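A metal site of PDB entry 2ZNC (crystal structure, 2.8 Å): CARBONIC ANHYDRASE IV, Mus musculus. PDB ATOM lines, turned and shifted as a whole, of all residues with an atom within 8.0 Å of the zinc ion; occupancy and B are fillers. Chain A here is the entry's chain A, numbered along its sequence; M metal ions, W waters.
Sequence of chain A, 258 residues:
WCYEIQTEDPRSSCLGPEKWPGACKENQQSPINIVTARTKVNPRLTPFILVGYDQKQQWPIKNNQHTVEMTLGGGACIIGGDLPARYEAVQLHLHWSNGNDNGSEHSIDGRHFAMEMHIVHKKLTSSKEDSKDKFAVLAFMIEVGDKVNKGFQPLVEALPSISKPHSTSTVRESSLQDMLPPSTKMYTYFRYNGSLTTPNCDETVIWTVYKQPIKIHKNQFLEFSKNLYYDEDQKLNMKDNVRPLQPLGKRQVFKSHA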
ATOM      1  N   TYR A   3       7.825  31.134  -5.980  1.00  0.00           N
ATOM      2  CA  TYR A   3       6.887  31.725  -6.924  1.00  0.00           C
ATOM      3  C   TYR A   3       5.798  32.480  -6.164  1.00  0.00           C
ATOM      4  O   TYR A   3       5.591  32.260  -4.972  1.00  0.00           O
ATOM      5  CB  TYR A   3       6.286  30.635  -7.817  1.00  0.00           C
ATOM      6  CG  TYR A   3       7.289  30.012  -8.767  1.00  0.00           C
ATOM      7  CD1 TYR A   3       7.779  30.729  -9.870  1.00  0.00           C
ATOM      8  CD2 TYR A   3       7.747  28.712  -8.591  1.00  0.00           C
ATOM      9  CE1 TYR A   3       8.693  30.162 -10.764  1.00  0.00           C
ATOM     10  CE2 TYR A   3       8.663  28.131  -9.483  1.00  0.00           C
ATOM     11  CZ  TYR A   3       9.133  28.864 -10.559  1.00  0.00           C
ATOM     12  OH  TYR A   3      10.004  28.293 -11.446  1.00  0.00           O
ATOM     13  N   THR A  67       9.783  21.800  -9.080  1.00  0.00           N
ATOM     14  CA  THR A  67       9.164  21.078 -10.185  1.00  0.00           C
ATOM     15  C   THR A  67       9.683  19.654 -10.160  1.00  0.00           C
ATOM     16  O   THR A  67      10.351  19.246  -9.213  1.00  0.00           O
ATOM     17  CB  THR A  67       9.530  21.732 -11.543  1.00  0.00           C
ATOM     18  OG1 THR A  67       8.872  21.047 -12.607  1.00  0.00           O
ATOM     19  CG2 THR A  67      11.045  21.714 -11.771  1.00  0.00           C
ATOM     20  N   GLN A  91      19.210  17.993 -18.271  1.00  0.00           N
ATOM     21  CA  GLN A  91      17.958  17.727 -17.540  1.00  0.00           C
ATOM     22  C   GLN A  91      16.697  18.199 -18.243  1.00  0.00           C
ATOM     23  O   GLN A  91      16.755  18.922 -19.239  1.00  0.00           O
ATOM     24  CB  GLN A  91      18.013  18.318 -16.128  1.00  0.00           C
ATOM     25  CG  GLN A  91      18.438  19.776 -16.053  1.00  0.00           C
ATOM     26  CD  GLN A  91      17.309  20.707 -15.698  1.00  0.00           C
ATOM     27  OE1 GLN A  91      16.158  20.301 -15.614  1.00  0.00           O
ATOM     28  NE2 GLN A  91      17.631  21.966 -15.475  1.00  0.00           N
ATOM     29  N   LEU A  92      15.554  17.796 -17.691  1.00  0.00           N
ATOM     30  CA  LEU A  92      14.234  18.133 -18.243  1.00  0.00           C
ATOM     31  C   LEU A  92      13.274  18.384 -17.078  1.00  0.00           C
ATOM     32  O   LEU A  92      13.402  17.767 -16.024  1.00  0.00           O
ATOM     33  CB  LEU A  92      13.753  16.937 -19.084  1.00  0.00           C
ATOM     34  CG  LEU A  92      12.368  16.699 -19.710  1.00  0.00           C
ATOM     35  CD1 LEU A  92      12.494  15.507 -20.641  1.00  0.00           C
ATOM     36  CD2 LEU A  92      11.284  16.439 -18.663  1.00  0.00           C
ATOM     37  N   HIS A  93      12.359  19.336 -17.262  1.00  0.00           N
ATOM     38  CA  HIS A  93      11.363  19.675 -16.244  1.00  0.00           C
ATOM     39  C   HIS A  93      10.195  20.391 -16.892  1.00  0.00           C
ATOM     40  O   HIS A  93      10.187  20.602 -18.107  1.00  0.00           O
ATOM     41  CB  HIS A  93      11.954  20.528 -15.112  1.00  0.00           C
ATOM     42  CG  HIS A  93      12.444  21.877 -15.545  1.00  0.00           C
ATOM     43  ND1 HIS A  93      13.768  22.176 -15.764  1.00  0.00           N
ATOM     44  CD2 HIS A  93      11.772  23.025 -15.780  1.00  0.00           C
ATOM     45  CE1 HIS A  93      13.850  23.468 -16.099  1.00  0.00           C
ATOM     46  NE2 HIS A  93      12.658  24.020 -16.122  1.00  0.00           N
ATOM     47  N   LEU A  94       9.175  20.742 -16.098  1.00  0.00           N
ATOM     48  CA  LEU A  94       8.002  21.410 -16.635  1.00  0.00           C
ATOM     49  C   LEU A  94       7.486  22.515 -15.716  1.00  0.00           C
ATOM     50  O   LEU A  94       7.894  22.620 -14.562  1.00  0.00           O
ATOM     51  CB  LEU A  94       6.869  20.404 -16.893  1.00  0.00           C
ATOM     52  CG  LEU A  94       7.090  19.258 -17.883  1.00  0.00           C
ATOM     53  CD1 LEU A  94       7.526  18.010 -17.139  1.00  0.00           C
ATOM     54  CD2 LEU A  94       5.802  18.972 -18.614  1.00  0.00           C
ATOM     55  N   HIS A  95       6.627  23.378 -16.277  1.00  0.00           N
ATOM     56  CA  HIS A  95       6.000  24.481 -15.555  1.00  0.00           C
ATOM     57  C   HIS A  95       4.535  24.314 -15.900  1.00  0.00           C
ATOM     58  O   HIS A  95       4.213  24.018 -17.058  1.00  0.00           O
ATOM     59  CB  HIS A  95       6.514  25.826 -16.041  1.00  0.00           C
ATOM     60  CG  HIS A  95       7.988  26.012 -15.857  1.00  0.00           C
ATOM     61  ND1 HIS A  95       8.557  26.566 -14.730  1.00  0.00           N
ATOM     62  CD2 HIS A  95       9.022  25.697 -16.665  1.00  0.00           C
ATOM     63  CE1 HIS A  95       9.884  26.578 -14.890  1.00  0.00           C
ATOM     64  NE2 HIS A  95      10.224  26.054 -16.057  1.00  0.00           N
ATOM     65  N   GLU A 105       4.898  29.279 -19.506  1.00  0.00           N
ATOM     66  CA  GLU A 105       5.629  30.503 -19.242  1.00  0.00           C
ATOM     67  C   GLU A 105       5.650  31.437 -20.465  1.00  0.00           C
ATOM     68  O   GLU A 105       5.220  32.585 -20.391  1.00  0.00           O
ATOM     69  CB  GLU A 105       7.040  30.194 -18.765  1.00  0.00           C
ATOM     70  CG  GLU A 105       7.071  29.502 -17.415  1.00  0.00           C
ATOM     71  CD  GLU A 105       8.458  29.496 -16.784  1.00  0.00           C
ATOM     72  OE1 GLU A 105       9.391  28.960 -17.406  1.00  0.00           O
ATOM     73  OE2 GLU A 105       8.613  30.044 -15.677  1.00  0.00           O
ATOM     74  N   HIS A 106       6.155  30.953 -21.597  1.00  0.00           N
ATOM     75  CA  HIS A 106       6.184  31.770 -22.800  1.00  0.00           C
ATOM     76  C   HIS A 106       4.750  31.802 -23.319  1.00  0.00           C
ATOM     77  O   HIS A 106       3.884  31.091 -22.792  1.00  0.00           O
ATOM     78  CB  HIS A 106       7.050  31.120 -23.899  1.00  0.00           C
ATOM     79  CG  HIS A 106       8.520  31.175 -23.631  1.00  0.00           C
ATOM     80  ND1 HIS A 106       9.176  30.267 -22.826  1.00  0.00           N
ATOM     81  CD2 HIS A 106       9.475  31.996 -24.129  1.00  0.00           C
ATOM     82  CE1 HIS A 106      10.463  30.521 -22.844  1.00  0.00           C
ATOM     83  NE2 HIS A 106      10.677  31.565 -23.620  1.00  0.00           N
ATOM     84  N   GLU A 116       4.516  23.707 -19.901  1.00  0.00           N
ATOM     85  CA  GLU A 116       5.676  23.987 -20.741  1.00  0.00           C
ATOM     86  C   GLU A 116       6.805  23.081 -20.257  1.00  0.00           C
ATOM     87  O   GLU A 116       7.087  23.017 -19.062  1.00  0.00           O
ATOM     88  CB  GLU A 116       6.090  25.450 -20.674  1.00  0.00           C
ATOM     89  CG  GLU A 116       7.147  25.810 -21.699  1.00  0.00           C
ATOM     90  CD  GLU A 116       7.329  27.299 -21.874  1.00  0.00           C
ATOM     91  OE1 GLU A 116       6.373  28.054 -21.628  1.00  0.00           O
ATOM     92  OE2 GLU A 116       8.425  27.725 -22.291  1.00  0.00           O
ATOM     93  N   MET A 117       7.375  22.314 -21.180  1.00  0.00           N
ATOM     94  CA  MET A 117       8.464  21.405 -20.866  1.00  0.00           C
ATOM     95  C   MET A 117       9.784  21.999 -21.309  1.00  0.00           C
ATOM     96  O   MET A 117       9.894  22.506 -22.435  1.00  0.00           O
ATOM     97  CB  MET A 117       8.237  20.061 -21.559  1.00  0.00           C
ATOM     98  CG  MET A 117       9.239  18.997 -21.199  1.00  0.00           C
ATOM     99  SD  MET A 117       8.654  17.426 -21.811  1.00  0.00           S
ATOM    100  CE  MET A 117       9.443  17.405 -23.394  1.00  0.00           C
ATOM    101  N   HIS A 118      10.775  21.960 -20.435  1.00  0.00           N
ATOM    102  CA  HIS A 118      12.083  22.504 -20.732  1.00  0.00           C
ATOM    103  C   HIS A 118      13.180  21.455 -20.753  1.00  0.00           C
ATOM    104  O   HIS A 118      13.363  20.723 -19.785  1.00  0.00           O
ATOM    105  CB  HIS A 118      12.443  23.582 -19.718  1.00  0.00           C
ATOM    106  CG  HIS A 118      11.672  24.850 -19.895  1.00  0.00           C
ATOM    107  ND1 HIS A 118      11.602  25.799 -18.902  1.00  0.00           N
ATOM    108  CD2 HIS A 118      10.964  25.275 -20.973  1.00  0.00           C
ATOM    109  CE1 HIS A 118      10.855  26.773 -19.399  1.00  0.00           C
ATOM    110  NE2 HIS A 118      10.449  26.495 -20.649  1.00  0.00           N
ATOM    111  N   ILE A 119      13.897  21.377 -21.868  1.00  0.00           N
ATOM    112  CA  ILE A 119      15.007  20.429 -21.993  1.00  0.00           C
ATOM    113  C   ILE A 119      16.268  21.298 -22.020  1.00  0.00           C
ATOM    114  O   ILE A 119      16.530  22.015 -22.988  1.00  0.00           O
ATOM    115  CB  ILE A 119      14.913  19.565 -23.278  1.00  0.00           C
ATOM    116  CG1 ILE A 119      13.481  19.025 -23.449  1.00  0.00           C
ATOM    117  CG2 ILE A 119      15.837  18.364 -23.166  1.00  0.00           C
ATOM    118  CD1 ILE A 119      13.262  18.280 -24.741  1.00  0.00           C
ATOM    119  N   VAL A 120      17.026  21.249 -20.931  1.00  0.00           N
ATOM    120  CA  VAL A 120      18.246  22.032 -20.792  1.00  0.00           C
ATOM    121  C   VAL A 120      19.456  21.288 -21.350  1.00  0.00           C
ATOM    122  O   VAL A 120      19.628  20.097 -21.127  1.00  0.00           O
ATOM    123  CB  VAL A 120      18.491  22.372 -19.293  1.00  0.00           C
ATOM    124  CG1 VAL A 120      19.682  23.318 -19.144  1.00  0.00           C
ATOM    125  CG2 VAL A 120      17.239  22.991 -18.670  1.00  0.00           C
ATOM    126  N   VAL A 137      18.140  25.618 -24.438  1.00  0.00           N
ATOM    127  CA  VAL A 137      16.932  25.083 -23.844  1.00  0.00           C
ATOM    128  C   VAL A 137      15.860  24.943 -24.922  1.00  0.00           C
ATOM    129  O   VAL A 137      15.540  25.912 -25.611  1.00  0.00           O
ATOM    130  CB  VAL A 137      16.397  25.952 -22.671  1.00  0.00           C
ATOM    131  CG1 VAL A 137      15.159  25.306 -22.074  1.00  0.00           C
ATOM    132  CG2 VAL A 137      17.460  26.112 -21.593  1.00  0.00           C
ATOM    133  N   ALA A 139      12.166  24.437 -25.578  1.00  0.00           N
ATOM    134  CA  ALA A 139      10.899  24.591 -24.874  1.00  0.00           C
ATOM    135  C   ALA A 139       9.723  24.145 -25.748  1.00  0.00           C
ATOM    136  O   ALA A 139       9.608  24.515 -26.920  1.00  0.00           O
ATOM    137  CB  ALA A 139      10.706  26.042 -24.441  1.00  0.00           C
ATOM    138  N   SER A 195      17.588  33.968 -20.883  1.00  0.00           N
ATOM    139  CA  SER A 195      18.149  33.472 -19.632  1.00  0.00           C
ATOM    140  C   SER A 195      17.260  32.395 -19.030  1.00  0.00           C
ATOM    141  O   SER A 195      16.190  32.075 -19.556  1.00  0.00           O
ATOM    142  CB  SER A 195      18.268  34.619 -18.636  1.00  0.00           C
ATOM    143  OG  SER A 195      16.983  35.140 -18.330  1.00  0.00           O
ATOM    144  N   LEU A 196      17.737  31.808 -17.924  1.00  0.00           N
ATOM    145  CA  LEU A 196      16.988  30.807 -17.175  1.00  0.00           C
ATOM    146  C   LEU A 196      15.794  31.578 -16.595  1.00  0.00           C
ATOM    147  O   LEU A 196      15.877  32.788 -16.399  1.00  0.00           O
ATOM    148  CB  LEU A 196      17.857  30.285 -16.020  1.00  0.00           C
ATOM    149  CG  LEU A 196      18.837  29.117 -16.156  1.00  0.00           C
ATOM    150  CD1 LEU A 196      19.506  29.074 -17.512  1.00  0.00           C
ATOM    151  CD2 LEU A 196      19.867  29.220 -15.054  1.00  0.00           C
ATOM    152  N   THR A 197      14.708  30.888 -16.303  1.00  0.00           N
ATOM    153  CA  THR A 197      13.533  31.535 -15.749  1.00  0.00           C
ATOM    154  C   THR A 197      13.419  31.298 -14.239  1.00  0.00           C
ATOM    155  O   THR A 197      12.341  31.400 -13.643  1.00  0.00           O
ATOM    156  CB  THR A 197      12.261  31.084 -16.485  1.00  0.00           C
ATOM    157  OG1 THR A 197      12.163  29.659 -16.433  1.00  0.00           O
ATOM    158  CG2 THR A 197      12.303  31.531 -17.933  1.00  0.00           C
ATOM    159  N   THR A 198      14.550  30.945 -13.630  1.00  0.00           N
ATOM    160  CA  THR A 198      14.643  30.686 -12.198  1.00  0.00           C
ATOM    161  C   THR A 198      16.012  31.207 -11.735  1.00  0.00           C
ATOM    162  O   THR A 198      16.984  31.130 -12.491  1.00  0.00           O
ATOM    163  CB  THR A 198      14.525  29.157 -11.875  1.00  0.00           C
ATOM    164  OG1 THR A 198      15.325  28.405 -12.795  1.00  0.00           O
ATOM    165  CG2 THR A 198      13.098  28.685 -11.985  1.00  0.00           C
ATOM    166  N   TRP A 207      17.343  30.195 -26.699  1.00  0.00           N
ATOM    167  CA  TRP A 207      16.029  29.553 -26.654  1.00  0.00           C
ATOM    168  C   TRP A 207      15.480  29.105 -27.998  1.00  0.00           C
ATOM    169  O   TRP A 207      15.651  29.775 -29.007  1.00  0.00           O
ATOM    170  CB  TRP A 207      14.991  30.484 -26.006  1.00  0.00           C
ATOM    171  CG  TRP A 207      15.067  30.562 -24.528  1.00  0.00           C
ATOM    172  CD1 TRP A 207      15.788  31.461 -23.798  1.00  0.00           C
ATOM    173  CD2 TRP A 207      14.398  29.725 -23.581  1.00  0.00           C
ATOM    174  NE1 TRP A 207      15.611  31.225 -22.460  1.00  0.00           N
ATOM    175  CE2 TRP A 207      14.769  30.170 -22.298  1.00  0.00           C
ATOM    176  CE3 TRP A 207      13.528  28.630 -23.696  1.00  0.00           C
ATOM    177  CZ2 TRP A 207      14.302  29.553 -21.127  1.00  0.00           C
ATOM    178  CZ3 TRP A 207      13.055  28.026 -22.536  1.00  0.00           C
ATOM    179  CH2 TRP A 207      13.444  28.493 -21.265  1.00  0.00           C
ATOM    180  N   ASN A 241       3.864  27.381 -10.941  1.00  0.00           N
ATOM    181  CA  ASN A 241       5.304  27.473 -10.779  1.00  0.00           C
ATOM    182  C   ASN A 241       5.884  28.099 -12.030  1.00  0.00           C
ATOM    183  O   ASN A 241       6.872  27.628 -12.601  1.00  0.00           O
ATOM    184  CB  ASN A 241       5.930  26.080 -10.508  1.00  0.00           C
ATOM    185  CG  ASN A 241       5.584  25.041 -11.556  1.00  0.00           C
ATOM    186  OD1 ASN A 241       4.664  25.202 -12.352  1.00  0.00           O
ATOM    187  ND2 ASN A 241       6.309  23.944 -11.540  1.00  0.00           N
HETATM  188 ZN    ZN M   1      12.141  25.885 -16.876  1.00  0.00          ZN
HETATM  189  O   HOH W   1      13.946  27.085 -15.796  1.00  0.00           O
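NE2 of His 118 is in hydrogen-bond range of OE2 of Glu 116 (2.9 Å). The backbone carbonyl oxygen of Glu 116 sits at hydrogen-bond distance from the backbone NH of His 95 (2.8 Å). The backbone carbonyl oxygen (O) of Asn 241 is in hydrogen-bond range of a ring nitrogen (ND1) of His 95 (2.9 Å). The side-chain carboxylate (OE1) of Glu 105 lies close to a ring nitrogen (NE2) of His 95 (3.3 Å). ND1 of His 93 is in hydrogen-bond range of OE1 of Gln 91. The side-chain carboxylate (OE1) of Glu 105 is in hydrogen-bond range of the side-chain hydroxyl (OG1) of Thr 197, 3.0 Å away.
Merely in contact with the zinc ion: Thr 197 (3.8 Å). Four residues have an atom within 4 Å of the zinc ion: His 93, His 95, His 118 and Thr 197. The nearest printed residue that does not touch the zinc ion is Glu 105 (4.2 Å).
The zinc ion is bound by a ring nitrogen (NE2) of His 93 (2.1 Å), a ring nitrogen (NE2) of His 95 (2.1 Å), a ring nitrogen (ND1) of His 118 (2.1 Å) and water W1 (2.4 Å). The zinc ion has four donor atoms within binding distance.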
